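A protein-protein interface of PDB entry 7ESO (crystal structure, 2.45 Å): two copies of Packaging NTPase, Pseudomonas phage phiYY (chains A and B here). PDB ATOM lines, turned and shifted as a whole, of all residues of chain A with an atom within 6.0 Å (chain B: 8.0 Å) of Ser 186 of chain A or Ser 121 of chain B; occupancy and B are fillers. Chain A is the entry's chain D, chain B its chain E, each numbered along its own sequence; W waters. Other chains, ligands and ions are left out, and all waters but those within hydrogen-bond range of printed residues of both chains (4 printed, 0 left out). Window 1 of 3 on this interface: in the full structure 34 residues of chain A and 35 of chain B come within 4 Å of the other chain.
Printed residues of chain B within 4 Å of Trp 169 of chain A: Leu 119 (3.5 Å) and Ser 121 (3.95 Å).
Of the printed residues of chain B, Val 185 of chain A touches Arg 123.
Of the printed residues of chain B, Asn 212 of chain A touches Leu 119, Leu 120, Ser 121 and Ser 232.
Of the printed residues of chain A, Leu 119 of chain B touches Trp 169, Leu 188 and Asn 212.
Printed residues of chain A within 4 Å of Pro 124 of chain B: Glu 171 (3.5 Å) and Ala 184 (3.5 Å).
The nearest residue of chain A that does not touch Ser 121 of chain B is Asp 187 of chain A (4.7 Å).
The nearest printed residue of chain A that does not touch Pro 118 of chain B is Trp 169 of chain A (4.5 Å).
Among the printed residues, merely in contact across the chains: Trp 169 of chain A with Leu 119 of chain B (3.5 Å), Trp 169 of chain A with Ser 121 of chain B (3.95 Å), Gly 170 of chain A with Ser 121 of chain B (3.5 Å), Gly 170 of chain A with Thr 235 of chain B (3.4 Å), Glu 171 of chain A with Pro 124 of chain B (3.5 Å), Glu 171 of chain A with Thr 235 of chain B (3.8 Å), Ala 184 of chain A with Arg 123 of chain B (3.6 Å), Ala 184 of chain A with Pro 124 of chain B (3.5 Å), Val 185 of chain A with Arg 123 of chain B (3.2 Å), Ser 186 of chain A with Leu 120 of chain B (3.5 Å), Ser 186 of chain A with Arg 123 of chain B (3.8 Å), Asp 187 of chain A with Tyr 117 of chain B (3.1 Å), Asp 187 of chain A with Pro 118 of chain B (3.3 Å), Leu 188 of chain A with Leu 119 of chain B (3.7 Å), Asn 212 of chain A with Leu 120 of chain B (3.8 Å), Asn 212 of chain A with Ser 121 of chain B (3.1 Å) and Asn 212 of chain A with Ser 232 of chain B (3.3 Å).
Of the 11 printed residues of chain A, 9 touch a printed residue of chain B.
Hydrophobic or aromatic side chains of chain A within 4 Å of the printed part of chain B: Trp 169, Ala 184 and Leu 188.
Of the 22 printed residues of chain B, 10 touch a printed residue of chain A.
Hydrophobic or aromatic side chains of chain B that line the printed part of chain A: Tyr 117, Leu 119, Leu 120 and Pro 124.
OD1 of Asp 187 of chain A is in hydrogen-bond range of N of Glu 190 of chain A (3.1 Å).
ND2 of Asn 239 of chain B sits at hydrogen-bond distance from O of Val 122 of chain B (3.0 Å).
NE of Arg 123 of chain B lies within salt-bridge range of OE2 of Glu 125 of chain B (2.6 Å).
The backbone carbonyl oxygen (O) of Ser 186 of chain A sits at hydrogen-bond distance from the indole nitrogen (NE1) of Trp 169 of chain A (3.3 Å).
The backbone NH (N) of Ser 186 of chain A lies within hydrogen-bond range of the side-chain carboxylate (OE1) of Glu 190 of chain A, 2.7 Å away.
The backbone carbonyl oxygen (O) of Arg 168 of chain A is in hydrogen-bond range of the backbone NH (N) of Val 185 of chain A.
Water W2 lies within hydrogen-bond range of the side-chain hydroxyl (OG) of Ser 121 of chain B, the backbone carbonyl oxygen (O) of Ser 232 of chain B and the side-chain amide nitrogen (ND2) of Asn 212 of chain A.
Water W3 lies within hydrogen-bond range of N of Gly 170 of chain A (2.7 Å), O of Val 122 of chain B (2.8 Å), O of Val 185 of chain A (2.8 Å) and OG of Ser 121 of chain B (3.3 Å).
Water W1 lies within hydrogen-bond range of NH2 of Arg 243 of chain B (2.8 Å), N of Arg 123 of chain B (2.9 Å) and OG of Ser 186 of chain A (3.1 Å).
Water W4 lies within hydrogen-bond range of O of Leu 120 of chain B (2.8 Å), ND2 of Asn 212 of chain A (3.5 Å) and O of Ser 232 of chain B (3.5 Å).
No position is printed for both chains.
The backbone carbonyl oxygen of Leu 119 of chain B lies within hydrogen-bond range of the side-chain amide nitrogen of Asn 212 of chain A (3.3 Å).
O of Ser 186 of chain A is in hydrogen-bond range of N of Ser 121 of chain B (2.6 Å).
O of Glu 171 of chain A lies within hydrogen-bond range of ND2 of Asn 239 of chain B, at 3.0 Å.
O of Pro 118 of chain B sits at hydrogen-bond distance from N of Leu 188 of chain A (3.0 Å).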
ATOM      1  N   ARG A 168       5.777  -9.766  17.962  1.00  0.00           N
ATOM      2  CA  ARG A 168       6.565 -10.224  16.825  1.00  0.00           C
ATOM      3  C   ARG A 168       7.070 -11.641  17.077  1.00  0.00           C
ATOM      4  O   ARG A 168       7.808 -11.886  18.038  1.00  0.00           O
ATOM      5  CB  ARG A 168       7.720  -9.265  16.551  1.00  0.00           C
ATOM      6  CG  ARG A 168       7.268  -7.916  15.977  1.00  0.00           C
ATOM      7  CD  ARG A 168       7.059  -7.994  14.466  1.00  0.00           C
ATOM      8  NE  ARG A 168       8.332  -8.096  13.755  1.00  0.00           N
ATOM      9  CZ  ARG A 168       8.450  -8.420  12.473  1.00  0.00           C
ATOM     10  NH1 ARG A 168       7.370  -8.675  11.749  1.00  0.00           N
ATOM     11  NH2 ARG A 168       9.649  -8.489  11.913  1.00  0.00           N
ATOM     12  N   TRP A 169       6.681 -12.566  16.204  1.00  0.00           N
ATOM     13  CA  TRP A 169       7.005 -13.972  16.382  1.00  0.00           C
ATOM     14  C   TRP A 169       7.231 -14.611  15.022  1.00  0.00           C
ATOM     15  O   TRP A 169       6.427 -14.415  14.105  1.00  0.00           O
ATOM     16  CB  TRP A 169       5.878 -14.678  17.129  1.00  0.00           C
ATOM     17  CG  TRP A 169       6.061 -16.137  17.272  1.00  0.00           C
ATOM     18  CD1 TRP A 169       7.189 -16.791  17.674  1.00  0.00           C
ATOM     19  CD2 TRP A 169       5.072 -17.143  17.041  1.00  0.00           C
ATOM     20  NE1 TRP A 169       6.966 -18.147  17.692  1.00  0.00           N
ATOM     21  CE2 TRP A 169       5.671 -18.388  17.312  1.00  0.00           C
ATOM     22  CE3 TRP A 169       3.739 -17.111  16.624  1.00  0.00           C
ATOM     23  CZ2 TRP A 169       4.984 -19.593  17.174  1.00  0.00           C
ATOM     24  CZ3 TRP A 169       3.054 -18.309  16.493  1.00  0.00           C
ATOM     25  CH2 TRP A 169       3.679 -19.533  16.767  1.00  0.00           C
ATOM     26  N   GLY A 170       8.336 -15.348  14.891  1.00  0.00           N
ATOM     27  CA  GLY A 170       8.628 -16.145  13.711  1.00  0.00           C
ATOM     28  C   GLY A 170       8.950 -15.387  12.441  1.00  0.00           C
ATOM     29  O   GLY A 170       8.911 -15.978  11.361  1.00  0.00           O
ATOM     30  N   GLU A 171       9.278 -14.106  12.530  1.00  0.00           N
ATOM     31  CA  GLU A 171       9.561 -13.307  11.359  1.00  0.00           C
ATOM     32  C   GLU A 171      10.999 -12.801  11.409  1.00  0.00           C
ATOM     33  O   GLU A 171      11.539 -12.574  12.497  1.00  0.00           O
ATOM     34  CB  GLU A 171       8.592 -12.121  11.269  1.00  0.00           C
ATOM     35  CG  GLU A 171       7.158 -12.525  10.933  1.00  0.00           C
ATOM     36  CD  GLU A 171       7.002 -12.951   9.480  1.00  0.00           C
ATOM     37  OE1 GLU A 171       7.827 -12.519   8.643  1.00  0.00           O
ATOM     38  OE2 GLU A 171       6.059 -13.716   9.178  1.00  0.00           O
ATOM     39  N   ALA A 184       8.987  -8.782  21.227  1.00  0.00           N
ATOM     40  CA  ALA A 184       9.515  -9.947  20.527  1.00  0.00           C
ATOM     41  C   ALA A 184       9.397 -11.184  21.406  1.00  0.00           C
ATOM     42  O   ALA A 184       9.753 -11.147  22.588  1.00  0.00           O
ATOM     43  CB  ALA A 184      10.974  -9.720  20.127  1.00  0.00           C
ATOM     44  N   VAL A 185       8.895 -12.275  20.824  1.00  0.00           N
ATOM     45  CA  VAL A 185       8.754 -13.551  21.511  1.00  0.00           C
ATOM     46  C   VAL A 185       9.346 -14.648  20.633  1.00  0.00           C
ATOM     47  O   VAL A 185       9.665 -14.440  19.459  1.00  0.00           O
ATOM     48  CB  VAL A 185       7.288 -13.882  21.876  1.00  0.00           C
ATOM     49  CG1 VAL A 185       6.683 -12.802  22.790  1.00  0.00           C
ATOM     50  CG2 VAL A 185       6.448 -14.072  20.622  1.00  0.00           C
ATOM     51  N   SER A 186       9.466 -15.837  21.231  1.00  0.00           N
ATOM     52  CA  SER A 186      10.151 -16.976  20.641  1.00  0.00           C
ATOM     53  C   SER A 186       9.245 -18.159  20.323  1.00  0.00           C
ATOM     54  O   SER A 186       9.608 -18.972  19.461  1.00  0.00           O
ATOM     55  CB  SER A 186      11.249 -17.476  21.592  1.00  0.00           C
ATOM     56  OG  SER A 186      12.046 -16.406  22.049  1.00  0.00           O
ATOM     57  N   ASP A 187       8.103 -18.299  21.006  1.00  0.00           N
ATOM     58  CA  ASP A 187       7.293 -19.500  20.846  1.00  0.00           C
ATOM     59  C   ASP A 187       5.815 -19.157  21.048  1.00  0.00           C
ATOM     60  O   ASP A 187       5.456 -18.034  21.423  1.00  0.00           O
ATOM     61  CB  ASP A 187       7.837 -20.618  21.766  1.00  0.00           C
ATOM     62  CG  ASP A 187       7.640 -20.344  23.265  1.00  0.00           C
ATOM     63  OD1 ASP A 187       6.758 -19.563  23.676  1.00  0.00           O
ATOM     64  OD2 ASP A 187       8.488 -20.841  24.038  1.00  0.00           O
ATOM     65  N   LEU A 188       4.952 -20.133  20.730  1.00  0.00           N
ATOM     66  CA  LEU A 188       3.511 -19.881  20.693  1.00  0.00           C
ATOM     67  C   LEU A 188       2.937 -19.622  22.083  1.00  0.00           C
ATOM     68  O   LEU A 188       1.927 -18.921  22.205  1.00  0.00           O
ATOM     69  CB  LEU A 188       2.786 -21.054  20.030  1.00  0.00           C
ATOM     70  CG  LEU A 188       1.261 -20.998  19.885  1.00  0.00           C
ATOM     71  CD1 LEU A 188       0.819 -19.747  19.149  1.00  0.00           C
ATOM     72  CD2 LEU A 188       0.774 -22.226  19.142  1.00  0.00           C
ATOM     73  N   GLU A 190       4.386 -17.799  24.447  1.00  0.00           N
ATOM     74  CA  GLU A 190       4.600 -16.377  24.696  1.00  0.00           C
ATOM     75  C   GLU A 190       3.685 -15.527  23.821  1.00  0.00           C
ATOM     76  O   GLU A 190       3.089 -14.555  24.300  1.00  0.00           O
ATOM     77  CB  GLU A 190       6.074 -16.017  24.476  1.00  0.00           C
ATOM     78  CG  GLU A 190       7.042 -16.848  25.332  1.00  0.00           C
ATOM     79  CD  GLU A 190       8.509 -16.667  24.966  1.00  0.00           C
ATOM     80  OE1 GLU A 190       8.807 -16.131  23.878  1.00  0.00           O
ATOM     81  OE2 GLU A 190       9.375 -17.084  25.767  1.00  0.00           O
ATOM     82  N   ASN A 212       5.055 -19.476  11.740  1.00  0.00           N
ATOM     83  CA  ASN A 212       5.458 -20.799  12.223  1.00  0.00           C
ATOM     84  C   ASN A 212       4.277 -21.725  12.439  1.00  0.00           C
ATOM     85  O   ASN A 212       4.442 -22.947  12.438  1.00  0.00           O
ATOM     86  CB  ASN A 212       6.235 -20.718  13.531  1.00  0.00           C
ATOM     87  CG  ASN A 212       7.715 -20.611  13.318  1.00  0.00           C
ATOM     88  OD1 ASN A 212       8.230 -20.956  12.258  1.00  0.00           O
ATOM     89  ND2 ASN A 212       8.425 -20.219  14.360  1.00  0.00           N
ATOM     90  N   ILE B  61      20.739 -19.470  24.031  1.00  0.00           N
ATOM     91  CA  ILE B  61      19.689 -19.203  23.053  1.00  0.00           C
ATOM     92  C   ILE B  61      19.404 -20.487  22.287  1.00  0.00           C
ATOM     93  O   ILE B  61      20.303 -21.060  21.659  1.00  0.00           O
ATOM     94  CB  ILE B  61      20.058 -18.071  22.081  1.00  0.00           C
ATOM     95  CG1 ILE B  61      20.504 -16.807  22.820  1.00  0.00           C
ATOM     96  CG2 ILE B  61      18.862 -17.748  21.193  1.00  0.00           C
ATOM     97  CD1 ILE B  61      21.053 -15.713  21.870  1.00  0.00           C
ATOM     98  N   MET B  62      18.152 -20.924  22.323  1.00  0.00           N
ATOM     99  CA  MET B  62      17.755 -22.117  21.595  1.00  0.00           C
ATOM    100  C   MET B  62      17.580 -21.792  20.121  1.00  0.00           C
ATOM    101  O   MET B  62      17.054 -20.735  19.762  1.00  0.00           O
ATOM    102  CB  MET B  62      16.457 -22.685  22.163  1.00  0.00           C
ATOM    103  CG  MET B  62      16.671 -23.453  23.438  1.00  0.00           C
ATOM    104  SD  MET B  62      15.143 -23.931  24.254  1.00  0.00           S
ATOM    105  CE  MET B  62      14.247 -22.390  24.269  1.00  0.00           C
ATOM    106  N   ILE B  63      18.039 -22.701  19.274  1.00  0.00           N
ATOM    107  CA  ILE B  63      17.966 -22.568  17.827  1.00  0.00           C
ATOM    108  C   ILE B  63      17.207 -23.768  17.279  1.00  0.00           C
ATOM    109  O   ILE B  63      17.772 -24.852  17.127  1.00  0.00           O
ATOM    110  CB  ILE B  63      19.366 -22.476  17.197  1.00  0.00           C
ATOM    111  CG1 ILE B  63      20.289 -21.587  18.029  1.00  0.00           C
ATOM    112  CG2 ILE B  63      19.265 -22.003  15.754  1.00  0.00           C
ATOM    113  CD1 ILE B  63      21.684 -21.462  17.458  1.00  0.00           C
ATOM    114  N   PRO B  64      15.923 -23.611  16.953  1.00  0.00           N
ATOM    115  CA  PRO B  64      15.158 -24.713  16.341  1.00  0.00           C
ATOM    116  C   PRO B  64      15.480 -24.838  14.856  1.00  0.00           C
ATOM    117  O   PRO B  64      15.357 -23.875  14.093  1.00  0.00           O
ATOM    118  CB  PRO B  64      13.699 -24.300  16.571  1.00  0.00           C
ATOM    119  CG  PRO B  64      13.752 -22.796  16.550  1.00  0.00           C
ATOM    120  CD  PRO B  64      15.101 -22.401  17.136  1.00  0.00           C
ATOM    121  N   TYR B 117       8.379 -25.683  24.466  1.00  0.00           N
ATOM    122  CA  TYR B 117       8.469 -24.466  23.653  1.00  0.00           C
ATOM    123  C   TYR B 117       7.773 -24.695  22.313  1.00  0.00           C
ATOM    124  O   TYR B 117       8.434 -24.894  21.281  1.00  0.00           O
ATOM    125  CB  TYR B 117       9.928 -24.037  23.487  1.00  0.00           C
ATOM    126  CG  TYR B 117      10.592 -23.896  24.832  1.00  0.00           C
ATOM    127  CD1 TYR B 117      10.295 -22.817  25.654  1.00  0.00           C
ATOM    128  CD2 TYR B 117      11.457 -24.873  25.313  1.00  0.00           C
ATOM    129  CE1 TYR B 117      10.861 -22.694  26.905  1.00  0.00           C
ATOM    130  CE2 TYR B 117      12.039 -24.757  26.569  1.00  0.00           C
ATOM    131  CZ  TYR B 117      11.730 -23.666  27.361  1.00  0.00           C
ATOM    132  OH  TYR B 117      12.290 -23.532  28.609  1.00  0.00           O
ATOM    133  N   PRO B 118       6.439 -24.625  22.281  1.00  0.00           N
ATOM    134  CA  PRO B 118       5.711 -25.012  21.064  1.00  0.00           C
ATOM    135  C   PRO B 118       6.016 -24.080  19.899  1.00  0.00           C
ATOM    136  O   PRO B 118       6.071 -22.858  20.057  1.00  0.00           O
ATOM    137  CB  PRO B 118       4.240 -24.915  21.484  1.00  0.00           C
ATOM    138  CG  PRO B 118       4.233 -23.899  22.580  1.00  0.00           C
ATOM    139  CD  PRO B 118       5.548 -24.051  23.307  1.00  0.00           C
ATOM    140  N   LEU B 119       6.219 -24.685  18.724  1.00  0.00           N
ATOM    141  CA  LEU B 119       6.494 -23.973  17.478  1.00  0.00           C
ATOM    142  C   LEU B 119       7.640 -22.980  17.657  1.00  0.00           C
ATOM    143  O   LEU B 119       7.619 -21.862  17.134  1.00  0.00           O
ATOM    144  CB  LEU B 119       5.224 -23.298  16.943  1.00  0.00           C
ATOM    145  CG  LEU B 119       4.072 -24.286  16.693  1.00  0.00           C
ATOM    146  CD1 LEU B 119       2.772 -23.601  16.283  1.00  0.00           C
ATOM    147  CD2 LEU B 119       4.466 -25.325  15.648  1.00  0.00           C
ATOM    148  N   LEU B 120       8.669 -23.424  18.378  1.00  0.00           N
ATOM    149  CA  LEU B 120       9.779 -22.558  18.762  1.00  0.00           C
ATOM    150  C   LEU B 120      10.405 -21.862  17.562  1.00  0.00           C
ATOM    151  O   LEU B 120      10.645 -22.471  16.514  1.00  0.00           O
ATOM    152  CB  LEU B 120      10.840 -23.373  19.496  1.00  0.00           C
ATOM    153  CG  LEU B 120      12.107 -22.667  19.970  1.00  0.00           C
ATOM    154  CD1 LEU B 120      11.792 -21.541  20.951  1.00  0.00           C
ATOM    155  CD2 LEU B 120      13.031 -23.688  20.621  1.00  0.00           C
ATOM    156  N   SER B 121      10.654 -20.568  17.731  1.00  0.00           N
ATOM    157  CA  SER B 121      11.426 -19.764  16.792  1.00  0.00           C
ATOM    158  C   SER B 121      12.540 -19.095  17.597  1.00  0.00           C
ATOM    159  O   SER B 121      12.863 -19.504  18.719  1.00  0.00           O
ATOM    160  CB  SER B 121      10.526 -18.741  16.084  1.00  0.00           C
ATOM    161  OG  SER B 121      11.264 -17.938  15.181  1.00  0.00           O
ATOM    162  N   VAL B 122      13.129 -18.038  17.039  1.00  0.00           N
ATOM    163  CA  VAL B 122      14.071 -17.185  17.757  1.00  0.00           C
ATOM    164  C   VAL B 122      13.562 -15.751  17.672  1.00  0.00           C
ATOM    165  O   VAL B 122      13.027 -15.336  16.637  1.00  0.00           O
ATOM    166  CB  VAL B 122      15.505 -17.315  17.196  1.00  0.00           C
ATOM    167  CG1 VAL B 122      16.469 -16.420  17.950  1.00  0.00           C
ATOM    168  CG2 VAL B 122      15.968 -18.770  17.272  1.00  0.00           C
ATOM    169  N   ARG B 123      13.715 -14.976  18.792  1.00  0.00           N
ATOM    170  CA  ARG B 123      12.977 -13.729  18.634  1.00  0.00           C
ATOM    171  C   ARG B 123      13.804 -12.665  17.915  1.00  0.00           C
ATOM    172  O   ARG B 123      15.035 -12.639  18.029  1.00  0.00           O
ATOM    173  CB  ARG B 123      12.530 -13.200  19.991  1.00  0.00           C
ATOM    174  CG  ARG B 123      13.637 -13.003  20.991  1.00  0.00           C
ATOM    175  CD  ARG B 123      13.067 -12.409  22.272  1.00  0.00           C
ATOM    176  NE  ARG B 123      14.093 -11.745  23.066  1.00  0.00           N
ATOM    177  CZ  ARG B 123      14.561 -12.213  24.219  1.00  0.00           C
ATOM    178  NH1 ARG B 123      14.092 -13.352  24.714  1.00  0.00           N
ATOM    179  NH2 ARG B 123      15.493 -11.542  24.879  1.00  0.00           N
ATOM    180  N   PRO B 124      13.134 -11.766  17.166  1.00  0.00           N
ATOM    181  CA  PRO B 124      13.866 -10.708  16.452  1.00  0.00           C
ATOM    182  C   PRO B 124      14.355  -9.623  17.397  1.00  0.00           C
ATOM    183  O   PRO B 124      13.554  -8.894  17.989  1.00  0.00           O
ATOM    184  CB  PRO B 124      12.825 -10.156  15.463  1.00  0.00           C
ATOM    185  CG  PRO B 124      11.600 -11.022  15.610  1.00  0.00           C
ATOM    186  CD  PRO B 124      11.681 -11.657  16.953  1.00  0.00           C
ATOM    187  N   GLU B 125      15.668  -9.519  17.559  1.00  0.00           N
ATOM    188  CA  GLU B 125      16.278  -8.476  18.365  1.00  0.00           C
ATOM    189  C   GLU B 125      17.486  -7.921  17.639  1.00  0.00           C
ATOM    190  O   GLU B 125      18.079  -8.584  16.786  1.00  0.00           O
ATOM    191  CB  GLU B 125      16.715  -8.974  19.745  1.00  0.00           C
ATOM    192  CG  GLU B 125      15.663  -8.856  20.826  1.00  0.00           C
ATOM    193  CD  GLU B 125      16.145  -9.416  22.152  1.00  0.00           C
ATOM    194  OE1 GLU B 125      17.334  -9.808  22.241  1.00  0.00           O
ATOM    195  OE2 GLU B 125      15.343  -9.444  23.108  1.00  0.00           O
ATOM    196  N   SER B 232      11.427 -21.731   7.847  1.00  0.00           N
ATOM    197  CA  SER B 232      11.416 -21.378   9.261  1.00  0.00           C
ATOM    198  C   SER B 232      12.765 -21.662   9.914  1.00  0.00           C
ATOM    199  O   SER B 232      13.112 -21.019  10.910  1.00  0.00           O
ATOM    200  CB  SER B 232      10.273 -22.097   9.988  1.00  0.00           C
ATOM    201  OG  SER B 232      10.373 -23.501   9.859  1.00  0.00           O
ATOM    202  N   ALA B 233      13.549 -22.597   9.362  1.00  0.00           N
ATOM    203  CA  ALA B 233      14.863 -22.868   9.939  1.00  0.00           C
ATOM    204  C   ALA B 233      15.802 -21.694   9.716  1.00  0.00           C
ATOM    205  O   ALA B 233      16.577 -21.324  10.609  1.00  0.00           O
ATOM    206  CB  ALA B 233      15.462 -24.140   9.345  1.00  0.00           C
ATOM    207  N   MET B 234      15.734 -21.087   8.534  1.00  0.00           N
ATOM    208  CA  MET B 234      16.601 -19.955   8.245  1.00  0.00           C
ATOM    209  C   MET B 234      16.145 -18.699   8.966  1.00  0.00           C
ATOM    210  O   MET B 234      16.985 -17.897   9.385  1.00  0.00           O
ATOM    211  CB  MET B 234      16.655 -19.715   6.751  1.00  0.00           C
ATOM    212  CG  MET B 234      17.381 -20.827   6.034  1.00  0.00           C
ATOM    213  SD  MET B 234      17.285 -20.357   4.324  1.00  0.00           S
ATOM    214  CE  MET B 234      15.518 -20.554   4.016  1.00  0.00           C
ATOM    215  N   THR B 235      14.831 -18.497   9.110  1.00  0.00           N
ATOM    216  CA  THR B 235      14.361 -17.425   9.975  1.00  0.00           C
ATOM    217  C   THR B 235      14.910 -17.595  11.390  1.00  0.00           C
ATOM    218  O   THR B 235      15.314 -16.616  12.030  1.00  0.00           O
ATOM    219  CB  THR B 235      12.836 -17.384   9.968  1.00  0.00           C
ATOM    220  OG1 THR B 235      12.374 -17.137   8.634  1.00  0.00           O
ATOM    221  CG2 THR B 235      12.310 -16.288  10.892  1.00  0.00           C
ATOM    222  N   ALA B 236      14.983 -18.837  11.876  1.00  0.00           N
ATOM    223  CA  ALA B 236      15.524 -19.080  13.210  1.00  0.00           C
ATOM    224  C   ALA B 236      17.019 -18.774  13.268  1.00  0.00           C
ATOM    225  O   ALA B 236      17.482 -18.065  14.170  1.00  0.00           O
ATOM    226  CB  ALA B 236      15.242 -20.525  13.634  1.00  0.00           C
ATOM    227  N   ILE B 237      17.794 -19.293  12.311  1.00  0.00           N
ATOM    228  CA  ILE B 237      19.226 -18.999  12.299  1.00  0.00           C
ATOM    229  C   ILE B 237      19.474 -17.513  12.010  1.00  0.00           C
ATOM    230  O   ILE B 237      20.424 -16.920  12.545  1.00  0.00           O
ATOM    231  CB  ILE B 237      19.944 -19.939  11.303  1.00  0.00           C
ATOM    232  CG1 ILE B 237      19.825 -21.388  11.781  1.00  0.00           C
ATOM    233  CG2 ILE B 237      21.426 -19.596  11.178  1.00  0.00           C
ATOM    234  CD1 ILE B 237      20.170 -22.427  10.742  1.00  0.00           C
ATOM    235  N   ASN B 239      17.613 -14.966  13.021  1.00  0.00           N
ATOM    236  CA  ASN B 239      17.364 -14.176  14.217  1.00  0.00           C
ATOM    237  C   ASN B 239      18.362 -14.463  15.334  1.00  0.00           C
ATOM    238  O   ASN B 239      18.527 -13.620  16.222  1.00  0.00           O
ATOM    239  CB  ASN B 239      15.931 -14.402  14.703  1.00  0.00           C
ATOM    240  CG  ASN B 239      14.906 -13.722  13.808  1.00  0.00           C
ATOM    241  OD1 ASN B 239      15.260 -12.944  12.920  1.00  0.00           O
ATOM    242  ND2 ASN B 239      13.636 -14.020  14.032  1.00  0.00           N
ATOM    243  N   VAL B 240      19.041 -15.615  15.312  1.00  0.00           N
ATOM    244  CA  VAL B 240      20.146 -15.817  16.248  1.00  0.00           C
ATOM    245  C   VAL B 240      21.287 -14.866  15.919  1.00  0.00           C
ATOM    246  O   VAL B 240      21.850 -14.219  16.810  1.00  0.00           O
ATOM    247  CB  VAL B 240      20.629 -17.278  16.240  1.00  0.00           C
ATOM    248  CG1 VAL B 240      21.918 -17.384  17.032  1.00  0.00           C
ATOM    249  CG2 VAL B 240      19.572 -18.210  16.820  1.00  0.00           C
ATOM    250  N   ARG B 243      20.236 -11.467  17.121  1.00  0.00           N
ATOM    251  CA  ARG B 243      20.441 -11.215  18.547  1.00  0.00           C
ATOM    252  C   ARG B 243      21.919 -11.059  18.887  1.00  0.00           C
ATOM    253  O   ARG B 243      22.264 -10.340  19.832  1.00  0.00           O
ATOM    254  CB  ARG B 243      19.811 -12.332  19.376  1.00  0.00           C
ATOM    255  CG  ARG B 243      18.293 -12.417  19.196  1.00  0.00           C
ATOM    256  CD  ARG B 243      17.662 -13.430  20.127  1.00  0.00           C
ATOM    257  NE  ARG B 243      18.069 -13.187  21.502  1.00  0.00           N
ATOM    258  CZ  ARG B 243      17.720 -13.945  22.531  1.00  0.00           C
ATOM    259  NH1 ARG B 243      18.151 -13.638  23.743  1.00  0.00           N
ATOM    260  NH2 ARG B 243      16.945 -15.007  22.348  1.00  0.00           N
HETATM  261  O   HOH W   1      14.962 -16.403  21.010  1.00  0.00           O
HETATM  262  O   HOH W   2      11.401 -19.302  13.004  1.00  0.00           O
HETATM  263  O   HOH W   3      10.241 -15.291  16.857  1.00  0.00           O
HETATM  264  O   HOH W   4      11.414 -21.936  13.828  1.00  0.00           O
